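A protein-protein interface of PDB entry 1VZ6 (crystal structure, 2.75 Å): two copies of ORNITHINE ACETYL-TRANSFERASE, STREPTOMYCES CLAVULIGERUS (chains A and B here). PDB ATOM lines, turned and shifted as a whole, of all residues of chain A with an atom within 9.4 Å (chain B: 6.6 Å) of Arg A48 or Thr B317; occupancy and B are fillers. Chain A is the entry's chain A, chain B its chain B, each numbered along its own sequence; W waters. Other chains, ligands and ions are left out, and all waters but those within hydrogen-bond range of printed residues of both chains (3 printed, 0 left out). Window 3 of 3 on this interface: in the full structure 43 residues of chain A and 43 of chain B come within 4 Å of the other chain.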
ATOM      1  N   THR A  45       9.092   3.463   4.371  1.00  0.00           N
ATOM      2  CA  THR A  45       8.045   3.908   5.268  1.00  0.00           C
ATOM      3  C   THR A  45       8.648   4.018   6.662  1.00  0.00           C
ATOM      4  O   THR A  45       9.600   3.322   6.991  1.00  0.00           O
ATOM      5  CB  THR A  45       6.890   2.880   5.291  1.00  0.00           C
ATOM      6  OG1 THR A  45       5.900   3.271   6.256  1.00  0.00           O
ATOM      7  CG2 THR A  45       7.432   1.487   5.627  1.00  0.00           C
ATOM      8  N   ARG A  46       8.099   4.901   7.481  1.00  0.00           N
ATOM      9  CA  ARG A  46       8.591   5.061   8.834  1.00  0.00           C
ATOM     10  C   ARG A  46       7.489   4.596   9.767  1.00  0.00           C
ATOM     11  O   ARG A  46       7.454   4.928  10.950  1.00  0.00           O
ATOM     12  CB  ARG A  46       8.973   6.521   9.080  1.00  0.00           C
ATOM     13  CG  ARG A  46      10.158   6.944   8.224  1.00  0.00           C
ATOM     14  CD  ARG A  46      10.548   8.400   8.416  1.00  0.00           C
ATOM     15  NE  ARG A  46       9.643   9.336   7.749  1.00  0.00           N
ATOM     16  CZ  ARG A  46       9.783  10.663   7.779  1.00  0.00           C
ATOM     17  NH1 ARG A  46      10.795  11.216   8.444  1.00  0.00           N
ATOM     18  NH2 ARG A  46       8.911  11.442   7.147  1.00  0.00           N
ATOM     19  N   SER A  47       6.592   3.798   9.200  1.00  0.00           N
ATOM     20  CA  SER A  47       5.456   3.240   9.920  1.00  0.00           C
ATOM     21  C   SER A  47       5.839   2.491  11.195  1.00  0.00           C
ATOM     22  O   SER A  47       6.854   1.791  11.247  1.00  0.00           O
ATOM     23  CB  SER A  47       4.678   2.294   9.003  1.00  0.00           C
ATOM     24  OG  SER A  47       3.587   1.701   9.693  1.00  0.00           O
ATOM     25  N   ARG A  48       5.008   2.637  12.219  1.00  0.00           N
ATOM     26  CA  ARG A  48       5.239   1.970  13.490  1.00  0.00           C
ATOM     27  C   ARG A  48       4.997   0.472  13.311  1.00  0.00           C
ATOM     28  O   ARG A  48       5.402  -0.332  14.148  1.00  0.00           O
ATOM     29  CB  ARG A  48       4.285   2.514  14.555  1.00  0.00           C
ATOM     30  CG  ARG A  48       4.546   3.945  14.982  1.00  0.00           C
ATOM     31  CD  ARG A  48       5.659   3.992  16.002  1.00  0.00           C
ATOM     32  NE  ARG A  48       6.978   3.894  15.394  1.00  0.00           N
ATOM     33  CZ  ARG A  48       8.000   3.244  15.938  1.00  0.00           C
ATOM     34  NH1 ARG A  48       7.853   2.622  17.101  1.00  0.00           N
ATOM     35  NH2 ARG A  48       9.177   3.235  15.328  1.00  0.00           N
ATOM     36  N   PHE A  49       4.319   0.103  12.230  1.00  0.00           N
ATOM     37  CA  PHE A  49       4.045  -1.303  11.965  1.00  0.00           C
ATOM     38  C   PHE A  49       4.811  -1.790  10.742  1.00  0.00           C
ATOM     39  O   PHE A  49       4.391  -2.740  10.080  1.00  0.00           O
ATOM     40  CB  PHE A  49       2.542  -1.543  11.754  1.00  0.00           C
ATOM     41  CG  PHE A  49       1.820  -2.031  12.985  1.00  0.00           C
ATOM     42  CD1 PHE A  49       1.451  -1.147  13.997  1.00  0.00           C
ATOM     43  CD2 PHE A  49       1.513  -3.385  13.132  1.00  0.00           C
ATOM     44  CE1 PHE A  49       0.788  -1.601  15.131  1.00  0.00           C
ATOM     45  CE2 PHE A  49       0.851  -3.850  14.263  1.00  0.00           C
ATOM     46  CZ  PHE A  49       0.487  -2.954  15.265  1.00  0.00           C
ATOM     47  N   ALA A  50       5.927  -1.136  10.439  1.00  0.00           N
ATOM     48  CA  ALA A  50       6.737  -1.533   9.291  1.00  0.00           C
ATOM     49  C   ALA A  50       7.054  -3.024   9.372  1.00  0.00           C
ATOM     50  O   ALA A  50       7.306  -3.547  10.457  1.00  0.00           O
ATOM     51  CB  ALA A  50       8.022  -0.736   9.260  1.00  0.00           C
ATOM     52  N   GLY A  51       7.040  -3.703   8.226  1.00  0.00           N
ATOM     53  CA  GLY A  51       7.321  -5.129   8.207  1.00  0.00           C
ATOM     54  C   GLY A  51       8.798  -5.489   8.227  1.00  0.00           C
ATOM     55  O   GLY A  51       9.660  -4.646   7.957  1.00  0.00           O
ATOM     56  N   PRO A  52       9.128  -6.754   8.528  1.00  0.00           N
ATOM     57  CA  PRO A  52      10.537  -7.167   8.567  1.00  0.00           C
ATOM     58  C   PRO A  52      11.319  -6.848   7.283  1.00  0.00           C
ATOM     59  O   PRO A  52      12.502  -6.507   7.341  1.00  0.00           O
ATOM     60  CB  PRO A  52      10.448  -8.667   8.856  1.00  0.00           C
ATOM     61  CG  PRO A  52       9.150  -9.059   8.242  1.00  0.00           C
ATOM     62  CD  PRO A  52       8.234  -7.919   8.637  1.00  0.00           C
ATOM     63  N   VAL A  54      11.221  -4.303   5.421  1.00  0.00           N
ATOM     64  CA  VAL A  54      11.721  -2.935   5.470  1.00  0.00           C
ATOM     65  C   VAL A  54      12.973  -2.861   6.333  1.00  0.00           C
ATOM     66  O   VAL A  54      13.961  -2.221   5.963  1.00  0.00           O
ATOM     67  CB  VAL A  54      10.648  -1.955   6.009  1.00  0.00           C
ATOM     68  CG1 VAL A  54      11.221  -0.535   6.076  1.00  0.00           C
ATOM     69  CG2 VAL A  54       9.421  -1.975   5.094  1.00  0.00           C
ATOM     70  N   VAL A  55      12.936  -3.530   7.476  1.00  0.00           N
ATOM     71  CA  VAL A  55      14.084  -3.535   8.370  1.00  0.00           C
ATOM     72  C   VAL A  55      15.319  -4.095   7.674  1.00  0.00           C
ATOM     73  O   VAL A  55      16.419  -3.555   7.812  1.00  0.00           O
ATOM     74  CB  VAL A  55      13.799  -4.348   9.640  1.00  0.00           C
ATOM     75  CG1 VAL A  55      15.074  -4.535  10.433  1.00  0.00           C
ATOM     76  CG2 VAL A  55      12.759  -3.619  10.484  1.00  0.00           C
ATOM     77  N   ARG A  58      16.668  -1.482   5.100  1.00  0.00           N
ATOM     78  CA  ARG A  58      17.368  -0.353   5.700  1.00  0.00           C
ATOM     79  C   ARG A  58      18.828  -0.716   5.963  1.00  0.00           C
ATOM     80  O   ARG A  58      19.718   0.112   5.785  1.00  0.00           O
ATOM     81  CB  ARG A  58      16.692   0.089   7.007  1.00  0.00           C
ATOM     82  CG  ARG A  58      15.271   0.641   6.855  1.00  0.00           C
ATOM     83  CD  ARG A  58      15.100   1.945   7.640  1.00  0.00           C
ATOM     84  NE  ARG A  58      13.719   2.431   7.675  1.00  0.00           N
ATOM     85  CZ  ARG A  58      12.744   1.892   8.415  1.00  0.00           C
ATOM     86  NH1 ARG A  58      12.983   0.841   9.196  1.00  0.00           N
ATOM     87  NH2 ARG A  58      11.519   2.407   8.382  1.00  0.00           N
ATOM     88  N   VAL A  78       3.561  -8.697   6.708  1.00  0.00           N
ATOM     89  CA  VAL A  78       3.558  -7.723   7.787  1.00  0.00           C
ATOM     90  C   VAL A  78       2.758  -8.276   8.975  1.00  0.00           C
ATOM     91  O   VAL A  78       1.768  -8.989   8.784  1.00  0.00           O
ATOM     92  CB  VAL A  78       2.916  -6.392   7.315  1.00  0.00           C
ATOM     93  CG1 VAL A  78       2.733  -5.451   8.486  1.00  0.00           C
ATOM     94  CG2 VAL A  78       3.792  -5.743   6.246  1.00  0.00           C
ATOM     95  N   ALA A  79       3.192  -7.951  10.193  1.00  0.00           N
ATOM     96  CA  ALA A  79       2.512  -8.409  11.400  1.00  0.00           C
ATOM     97  C   ALA A  79       2.427  -9.922  11.402  1.00  0.00           C
ATOM     98  O   ALA A  79       1.394 -10.492  11.743  1.00  0.00           O
ATOM     99  CB  ALA A  79       1.110  -7.804  11.481  1.00  0.00           C
ATOM    100  N   THR A 218      -0.861   5.764   4.895  1.00  0.00           N
ATOM    101  CA  THR A 218       0.546   5.452   4.746  1.00  0.00           C
ATOM    102  C   THR A 218       0.773   3.991   5.050  1.00  0.00           C
ATOM    103  O   THR A 218       0.452   3.516   6.135  1.00  0.00           O
ATOM    104  CB  THR A 218       1.386   6.284   5.690  1.00  0.00           C
ATOM    105  OG1 THR A 218       1.094   7.665   5.469  1.00  0.00           O
ATOM    106  CG2 THR A 218       2.860   6.040   5.440  1.00  0.00           C
ATOM    107  N   SER A 219       1.343   3.296   4.076  1.00  0.00           N
ATOM    108  CA  SER A 219       1.620   1.869   4.162  1.00  0.00           C
ATOM    109  C   SER A 219       2.662   1.422   5.187  1.00  0.00           C
ATOM    110  O   SER A 219       3.438   2.215   5.715  1.00  0.00           O
ATOM    111  CB  SER A 219       2.039   1.362   2.783  1.00  0.00           C
ATOM    112  OG  SER A 219       2.305  -0.024   2.816  1.00  0.00           O
ATOM    113  N   THR A 220       2.664   0.118   5.440  1.00  0.00           N
ATOM    114  CA  THR A 220       3.589  -0.519   6.366  1.00  0.00           C
ATOM    115  C   THR A 220       4.725  -1.102   5.546  1.00  0.00           C
ATOM    116  O   THR A 220       5.647  -1.698   6.097  1.00  0.00           O
ATOM    117  CB  THR A 220       2.935  -1.712   7.076  1.00  0.00           C
ATOM    118  OG1 THR A 220       2.441  -2.622   6.083  1.00  0.00           O
ATOM    119  CG2 THR A 220       1.793  -1.269   7.959  1.00  0.00           C
ATOM    120  N   SER A 221       4.657  -0.924   4.228  1.00  0.00           N
ATOM    121  CA  SER A 221       5.650  -1.506   3.338  1.00  0.00           C
ATOM    122  C   SER A 221       6.260  -0.609   2.270  1.00  0.00           C
ATOM    123  O   SER A 221       7.058  -1.092   1.464  1.00  0.00           O
ATOM    124  CB  SER A 221       5.023  -2.720   2.661  1.00  0.00           C
ATOM    125  OG  SER A 221       4.286  -3.475   3.606  1.00  0.00           O
ATOM    126  N   ARG B 274       0.806   6.990  26.022  1.00  0.00           N
ATOM    127  CA  ARG B 274       1.693   7.640  26.971  1.00  0.00           C
ATOM    128  C   ARG B 274       0.951   8.748  27.703  1.00  0.00           C
ATOM    129  O   ARG B 274       1.370   9.197  28.768  1.00  0.00           O
ATOM    130  CB  ARG B 274       2.960   8.167  26.289  1.00  0.00           C
ATOM    131  CG  ARG B 274       2.841   9.449  25.529  1.00  0.00           C
ATOM    132  CD  ARG B 274       4.234   9.940  25.223  1.00  0.00           C
ATOM    133  NE  ARG B 274       4.248  10.979  24.200  1.00  0.00           N
ATOM    134  CZ  ARG B 274       4.637  10.794  22.942  1.00  0.00           C
ATOM    135  NH1 ARG B 274       5.051   9.600  22.528  1.00  0.00           N
ATOM    136  NH2 ARG B 274       4.623  11.817  22.095  1.00  0.00           N
ATOM    137  N   GLN B 278      -2.140  11.530  23.105  1.00  0.00           N
ATOM    138  CA  GLN B 278      -1.700  10.519  22.159  1.00  0.00           C
ATOM    139  C   GLN B 278      -2.787   9.476  21.930  1.00  0.00           C
ATOM    140  O   GLN B 278      -2.908   8.923  20.829  1.00  0.00           O
ATOM    141  CB  GLN B 278      -0.443   9.818  22.659  1.00  0.00           C
ATOM    142  CG  GLN B 278       0.088   8.787  21.682  1.00  0.00           C
ATOM    143  CD  GLN B 278       1.160   7.916  22.283  1.00  0.00           C
ATOM    144  OE1 GLN B 278       0.893   7.109  23.176  1.00  0.00           O
ATOM    145  NE2 GLN B 278       2.389   8.074  21.804  1.00  0.00           N
ATOM    146  N   ALA B 307      -4.115  -2.016  12.287  1.00  0.00           N
ATOM    147  CA  ALA B 307      -2.682  -2.003  12.576  1.00  0.00           C
ATOM    148  C   ALA B 307      -1.984  -0.975  11.666  1.00  0.00           C
ATOM    149  O   ALA B 307      -1.179  -0.156  12.127  1.00  0.00           O
ATOM    150  CB  ALA B 307      -2.102  -3.388  12.352  1.00  0.00           C
ATOM    151  N   ILE B 310      -2.805   2.420  12.968  1.00  0.00           N
ATOM    152  CA  ILE B 310      -2.044   2.765  14.163  1.00  0.00           C
ATOM    153  C   ILE B 310      -0.622   3.133  13.746  1.00  0.00           C
ATOM    154  O   ILE B 310      -0.059   4.114  14.225  1.00  0.00           O
ATOM    155  CB  ILE B 310      -1.988   1.584  15.153  1.00  0.00           C
ATOM    156  CG1 ILE B 310      -3.394   1.260  15.662  1.00  0.00           C
ATOM    157  CG2 ILE B 310      -1.079   1.926  16.317  1.00  0.00           C
ATOM    158  CD1 ILE B 310      -3.466   0.008  16.499  1.00  0.00           C
ATOM    159  N   GLY B 311      -0.059   2.348  12.833  1.00  0.00           N
ATOM    160  CA  GLY B 311       1.288   2.600  12.363  1.00  0.00           C
ATOM    161  C   GLY B 311       1.513   3.951  11.700  1.00  0.00           C
ATOM    162  O   GLY B 311       2.656   4.398  11.604  1.00  0.00           O
ATOM    163  N   LYS B 312       0.447   4.602  11.236  1.00  0.00           N
ATOM    164  CA  LYS B 312       0.575   5.911  10.586  1.00  0.00           C
ATOM    165  C   LYS B 312       1.049   6.994  11.558  1.00  0.00           C
ATOM    166  O   LYS B 312       1.504   8.053  11.137  1.00  0.00           O
ATOM    167  CB  LYS B 312      -0.750   6.338   9.936  1.00  0.00           C
ATOM    168  CG  LYS B 312      -1.195   5.436   8.795  1.00  0.00           C
ATOM    169  CD  LYS B 312      -2.248   6.092   7.918  1.00  0.00           C
ATOM    170  CE  LYS B 312      -3.494   6.459   8.696  1.00  0.00           C
ATOM    171  NZ  LYS B 312      -4.518   7.101   7.825  1.00  0.00           N
ATOM    172  N   CYS B 313       0.933   6.739  12.857  1.00  0.00           N
ATOM    173  CA  CYS B 313       1.399   7.703  13.848  1.00  0.00           C
ATOM    174  C   CYS B 313       2.899   7.470  14.002  1.00  0.00           C
ATOM    175  O   CYS B 313       3.401   7.150  15.084  1.00  0.00           O
ATOM    176  CB  CYS B 313       0.680   7.481  15.169  1.00  0.00           C
ATOM    177  SG  CYS B 313      -1.097   7.704  15.012  1.00  0.00           S
ATOM    178  N   SER B 314       3.604   7.632  12.887  1.00  0.00           N
ATOM    179  CA  SER B 314       5.038   7.414  12.828  1.00  0.00           C
ATOM    180  C   SER B 314       5.865   8.312  13.729  1.00  0.00           C
ATOM    181  O   SER B 314       7.040   8.041  13.942  1.00  0.00           O
ATOM    182  CB  SER B 314       5.519   7.561  11.391  1.00  0.00           C
ATOM    183  OG  SER B 314       5.185   8.840  10.895  1.00  0.00           O
ATOM    184  N   ASP B 315       5.284   9.384  14.253  1.00  0.00           N
ATOM    185  CA  ASP B 315       6.066  10.229  15.131  1.00  0.00           C
ATOM    186  C   ASP B 315       5.969   9.765  16.570  1.00  0.00           C
ATOM    187  O   ASP B 315       6.733  10.199  17.426  1.00  0.00           O
ATOM    188  CB  ASP B 315       5.658  11.688  15.000  1.00  0.00           C
ATOM    189  CG  ASP B 315       6.221  12.324  13.748  1.00  0.00           C
ATOM    190  OD1 ASP B 315       7.187  11.757  13.189  1.00  0.00           O
ATOM    191  OD2 ASP B 315       5.716  13.385  13.321  1.00  0.00           O
ATOM    192  N   ASP B 316       5.036   8.863  16.834  1.00  0.00           N
ATOM    193  CA  ASP B 316       4.885   8.328  18.170  1.00  0.00           C
ATOM    194  C   ASP B 316       5.750   7.084  18.265  1.00  0.00           C
ATOM    195  O   ASP B 316       5.257   5.955  18.339  1.00  0.00           O
ATOM    196  CB  ASP B 316       3.418   8.013  18.440  1.00  0.00           C
ATOM    197  CG  ASP B 316       2.575   9.264  18.490  1.00  0.00           C
ATOM    198  OD1 ASP B 316       2.064   9.697  17.435  1.00  0.00           O
ATOM    199  OD2 ASP B 316       2.449   9.833  19.589  1.00  0.00           O
ATOM    200  N   THR B 317       7.059   7.318  18.267  1.00  0.00           N
ATOM    201  CA  THR B 317       8.048   6.243  18.309  1.00  0.00           C
ATOM    202  C   THR B 317       7.991   5.341  19.533  1.00  0.00           C
ATOM    203  O   THR B 317       8.714   4.356  19.593  1.00  0.00           O
ATOM    204  CB  THR B 317       9.472   6.801  18.179  1.00  0.00           C
ATOM    205  OG1 THR B 317       9.791   7.580  19.336  1.00  0.00           O
ATOM    206  CG2 THR B 317       9.574   7.680  16.946  1.00  0.00           C
ATOM    207  N   ASP B 318       7.149   5.661  20.510  1.00  0.00           N
ATOM    208  CA  ASP B 318       7.052   4.792  21.674  1.00  0.00           C
ATOM    209  C   ASP B 318       5.997   3.717  21.462  1.00  0.00           C
ATOM    210  O   ASP B 318       5.763   2.875  22.330  1.00  0.00           O
ATOM    211  CB  ASP B 318       6.781   5.590  22.965  1.00  0.00           C
ATOM    212  CG  ASP B 318       5.680   6.633  22.821  1.00  0.00           C
ATOM    213  OD1 ASP B 318       5.345   7.024  21.680  1.00  0.00           O
ATOM    214  OD2 ASP B 318       5.165   7.086  23.872  1.00  0.00           O
ATOM    215  N   ILE B 319       5.366   3.743  20.291  1.00  0.00           N
ATOM    216  CA  ILE B 319       4.356   2.749  19.968  1.00  0.00           C
ATOM    217  C   ILE B 319       5.090   1.539  19.408  1.00  0.00           C
ATOM    218  O   ILE B 319       5.613   1.581  18.295  1.00  0.00           O
ATOM    219  CB  ILE B 319       3.343   3.257  18.915  1.00  0.00           C
ATOM    220  CG1 ILE B 319       2.558   4.448  19.469  1.00  0.00           C
ATOM    221  CG2 ILE B 319       2.372   2.135  18.547  1.00  0.00           C
ATOM    222  CD1 ILE B 319       1.478   4.954  18.538  1.00  0.00           C
ATOM    223  N   ASP B 320       5.129   0.467  20.193  1.00  0.00           N
ATOM    224  CA  ASP B 320       5.808  -0.751  19.795  1.00  0.00           C
ATOM    225  C   ASP B 320       4.842  -1.766  19.206  1.00  0.00           C
ATOM    226  O   ASP B 320       3.963  -2.301  19.883  1.00  0.00           O
ATOM    227  CB  ASP B 320       6.531  -1.367  20.992  1.00  0.00           C
ATOM    228  CG  ASP B 320       7.438  -2.520  20.602  1.00  0.00           C
ATOM    229  OD1 ASP B 320       7.220  -3.134  19.535  1.00  0.00           O
ATOM    230  OD2 ASP B 320       8.368  -2.824  21.373  1.00  0.00           O
ATOM    231  N   GLN B 321       5.036  -2.015  17.921  1.00  0.00           N
ATOM    232  CA  GLN B 321       4.253  -2.954  17.145  1.00  0.00           C
ATOM    233  C   GLN B 321       4.036  -4.293  17.867  1.00  0.00           C
ATOM    234  O   GLN B 321       3.045  -4.988  17.635  1.00  0.00           O
ATOM    235  CB  GLN B 321       4.995  -3.153  15.831  1.00  0.00           C
ATOM    236  CG  GLN B 321       4.574  -4.307  14.978  1.00  0.00           C
ATOM    237  CD  GLN B 321       5.437  -4.415  13.735  1.00  0.00           C
ATOM    238  OE1 GLN B 321       5.186  -5.248  12.868  1.00  0.00           O
ATOM    239  NE2 GLN B 321       6.460  -3.566  13.641  1.00  0.00           N
ATOM    240  N   GLU B 322       4.958  -4.638  18.758  1.00  0.00           N
ATOM    241  CA  GLU B 322       4.889  -5.895  19.488  1.00  0.00           C
ATOM    242  C   GLU B 322       4.056  -5.841  20.749  1.00  0.00           C
ATOM    243  O   GLU B 322       3.493  -6.848  21.153  1.00  0.00           O
ATOM    244  CB  GLU B 322       6.290  -6.351  19.855  1.00  0.00           C
ATOM    245  CG  GLU B 322       7.249  -6.326  18.693  1.00  0.00           C
ATOM    246  CD  GLU B 322       7.838  -7.685  18.409  1.00  0.00           C
ATOM    247  OE1 GLU B 322       7.066  -8.603  18.050  1.00  0.00           O
ATOM    248  OE2 GLU B 322       9.071  -7.836  18.551  1.00  0.00           O
ATOM    249  N   ILE B 368       1.968   1.614  26.806  1.00  0.00           N
ATOM    250  CA  ILE B 368       3.059   2.559  26.989  1.00  0.00           C
ATOM    251  C   ILE B 368       2.932   3.160  28.382  1.00  0.00           C
ATOM    252  O   ILE B 368       3.880   3.128  29.163  1.00  0.00           O
ATOM    253  CB  ILE B 368       2.999   3.700  25.964  1.00  0.00           C
ATOM    254  CG1 ILE B 368       3.238   3.154  24.556  1.00  0.00           C
ATOM    255  CG2 ILE B 368       4.020   4.774  26.320  1.00  0.00           C
ATOM    256  CD1 ILE B 368       3.200   4.222  23.480  1.00  0.00           C
HETATM  257  O   HOH W   1       6.962  -0.598  16.204  1.00  0.00           O
HETATM  258  O   HOH W   2       5.348  -6.153  10.627  1.00  0.00           O
HETATM  259  O   HOH W   3       8.287   5.714  13.364  1.00  0.00           O
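Of the 17 printed residues of chain B, 9 touch a printed residue of chain A. Hydrophobic or aromatic side chains of chain B that line the printed part of chain A: Ala B307 and Ile B319. Hydrophobic or aromatic side chains of chain A within 4 Å of the printed part of chain B: Phe A49. Among the printed residues, no Asp or Glu carboxylate lies within 4 Å of a Lys or Arg side-chain nitrogen of the other chain.
The side-chain hydroxyl (OG1) of Thr A45 is in hydrogen-bond range of the backbone NH (N) of Ser A47 (3.1 Å). OG of Ser A47 sits close to N of Phe A49 (3.1 Å). NH2 of Arg B274 lies within salt-bridge range of OD2 of Asp B316. The side-chain amide nitrogen of Gln B278 is in hydrogen-bond range of the side-chain carboxylate of Asp B316.
OG of Ser A47 is in hydrogen-bond range of O of Gly B311 (3.4 Å). The backbone NH of Arg A48 is in hydrogen-bond range of the backbone carbonyl oxygen of Gly B311 (3.0 Å). NH1 of Arg A48 sits at hydrogen-bond distance from O of Thr B317 (3.2 Å). The guanidinium group (NH1) of Arg A48 is in hydrogen-bond range of the backbone carbonyl oxygen (O) of Ile B319 (2.7 Å). The backbone carbonyl oxygen (O) of Arg A48 sits close to the side-chain amide nitrogen (NE2) of Gln B321 (3.4 Å). O of Ala A50 sits at hydrogen-bond distance from NE2 of Gln B321 (3.3 Å).
No position is printed for both chains.
Printed residues of chain B within 4 Å of Thr A218: Lys B312. Of chain A, only Ser A47, Arg A48 and Phe A49 come within 4 Å of Gly B311. Asp B315 touches none of the printed residues of chain A. Of the printed residues of chain A, Asp B316 touches Arg A48 (3.1 Å). Of chain A, only Arg A48 comes within 4 Å of Ile B319. Of the printed residues of chain A, Gln B321 touches Arg A48 (3.3 Å), Phe A49 (3.7 Å) and Ala A50 (3.3 Å). Ile B368 touches none of the printed residues of chain A. The nearest residue of chain B that does not touch Arg A48 is Ser B314 (4.1 Å). The nearest printed residue of chain A that does not touch Asp B316 is Arg A46 (7.5 Å).
Ser B314 touches Arg A46 (CB to O, 3.3 Å). Cys B313 touches Arg A48 (O to CG, 3.4 Å). Asp B316 touches Arg A48 (O to CD, 3.1 Å). Phe A49 touches Ala B307. N of Phe A49 touches CA of Gly B311, at 3.9 Å. Phe A49 touches Gln B321 (CD2 to CG, 3.7 Å). Thr A218 touches Lys B312 (N to CD, 3.3 Å).
Water W2 lies within hydrogen-bond range of OE1 of Gln B321, N of Ala A79 and O of Ala A50. Water W1 lies within hydrogen-bond range of O of Arg A48, N of Gln B321 and O of Ile B319. Water W3 lies within hydrogen-bond range of O of Arg A46, O of Ser B314 and NE of Arg A48.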
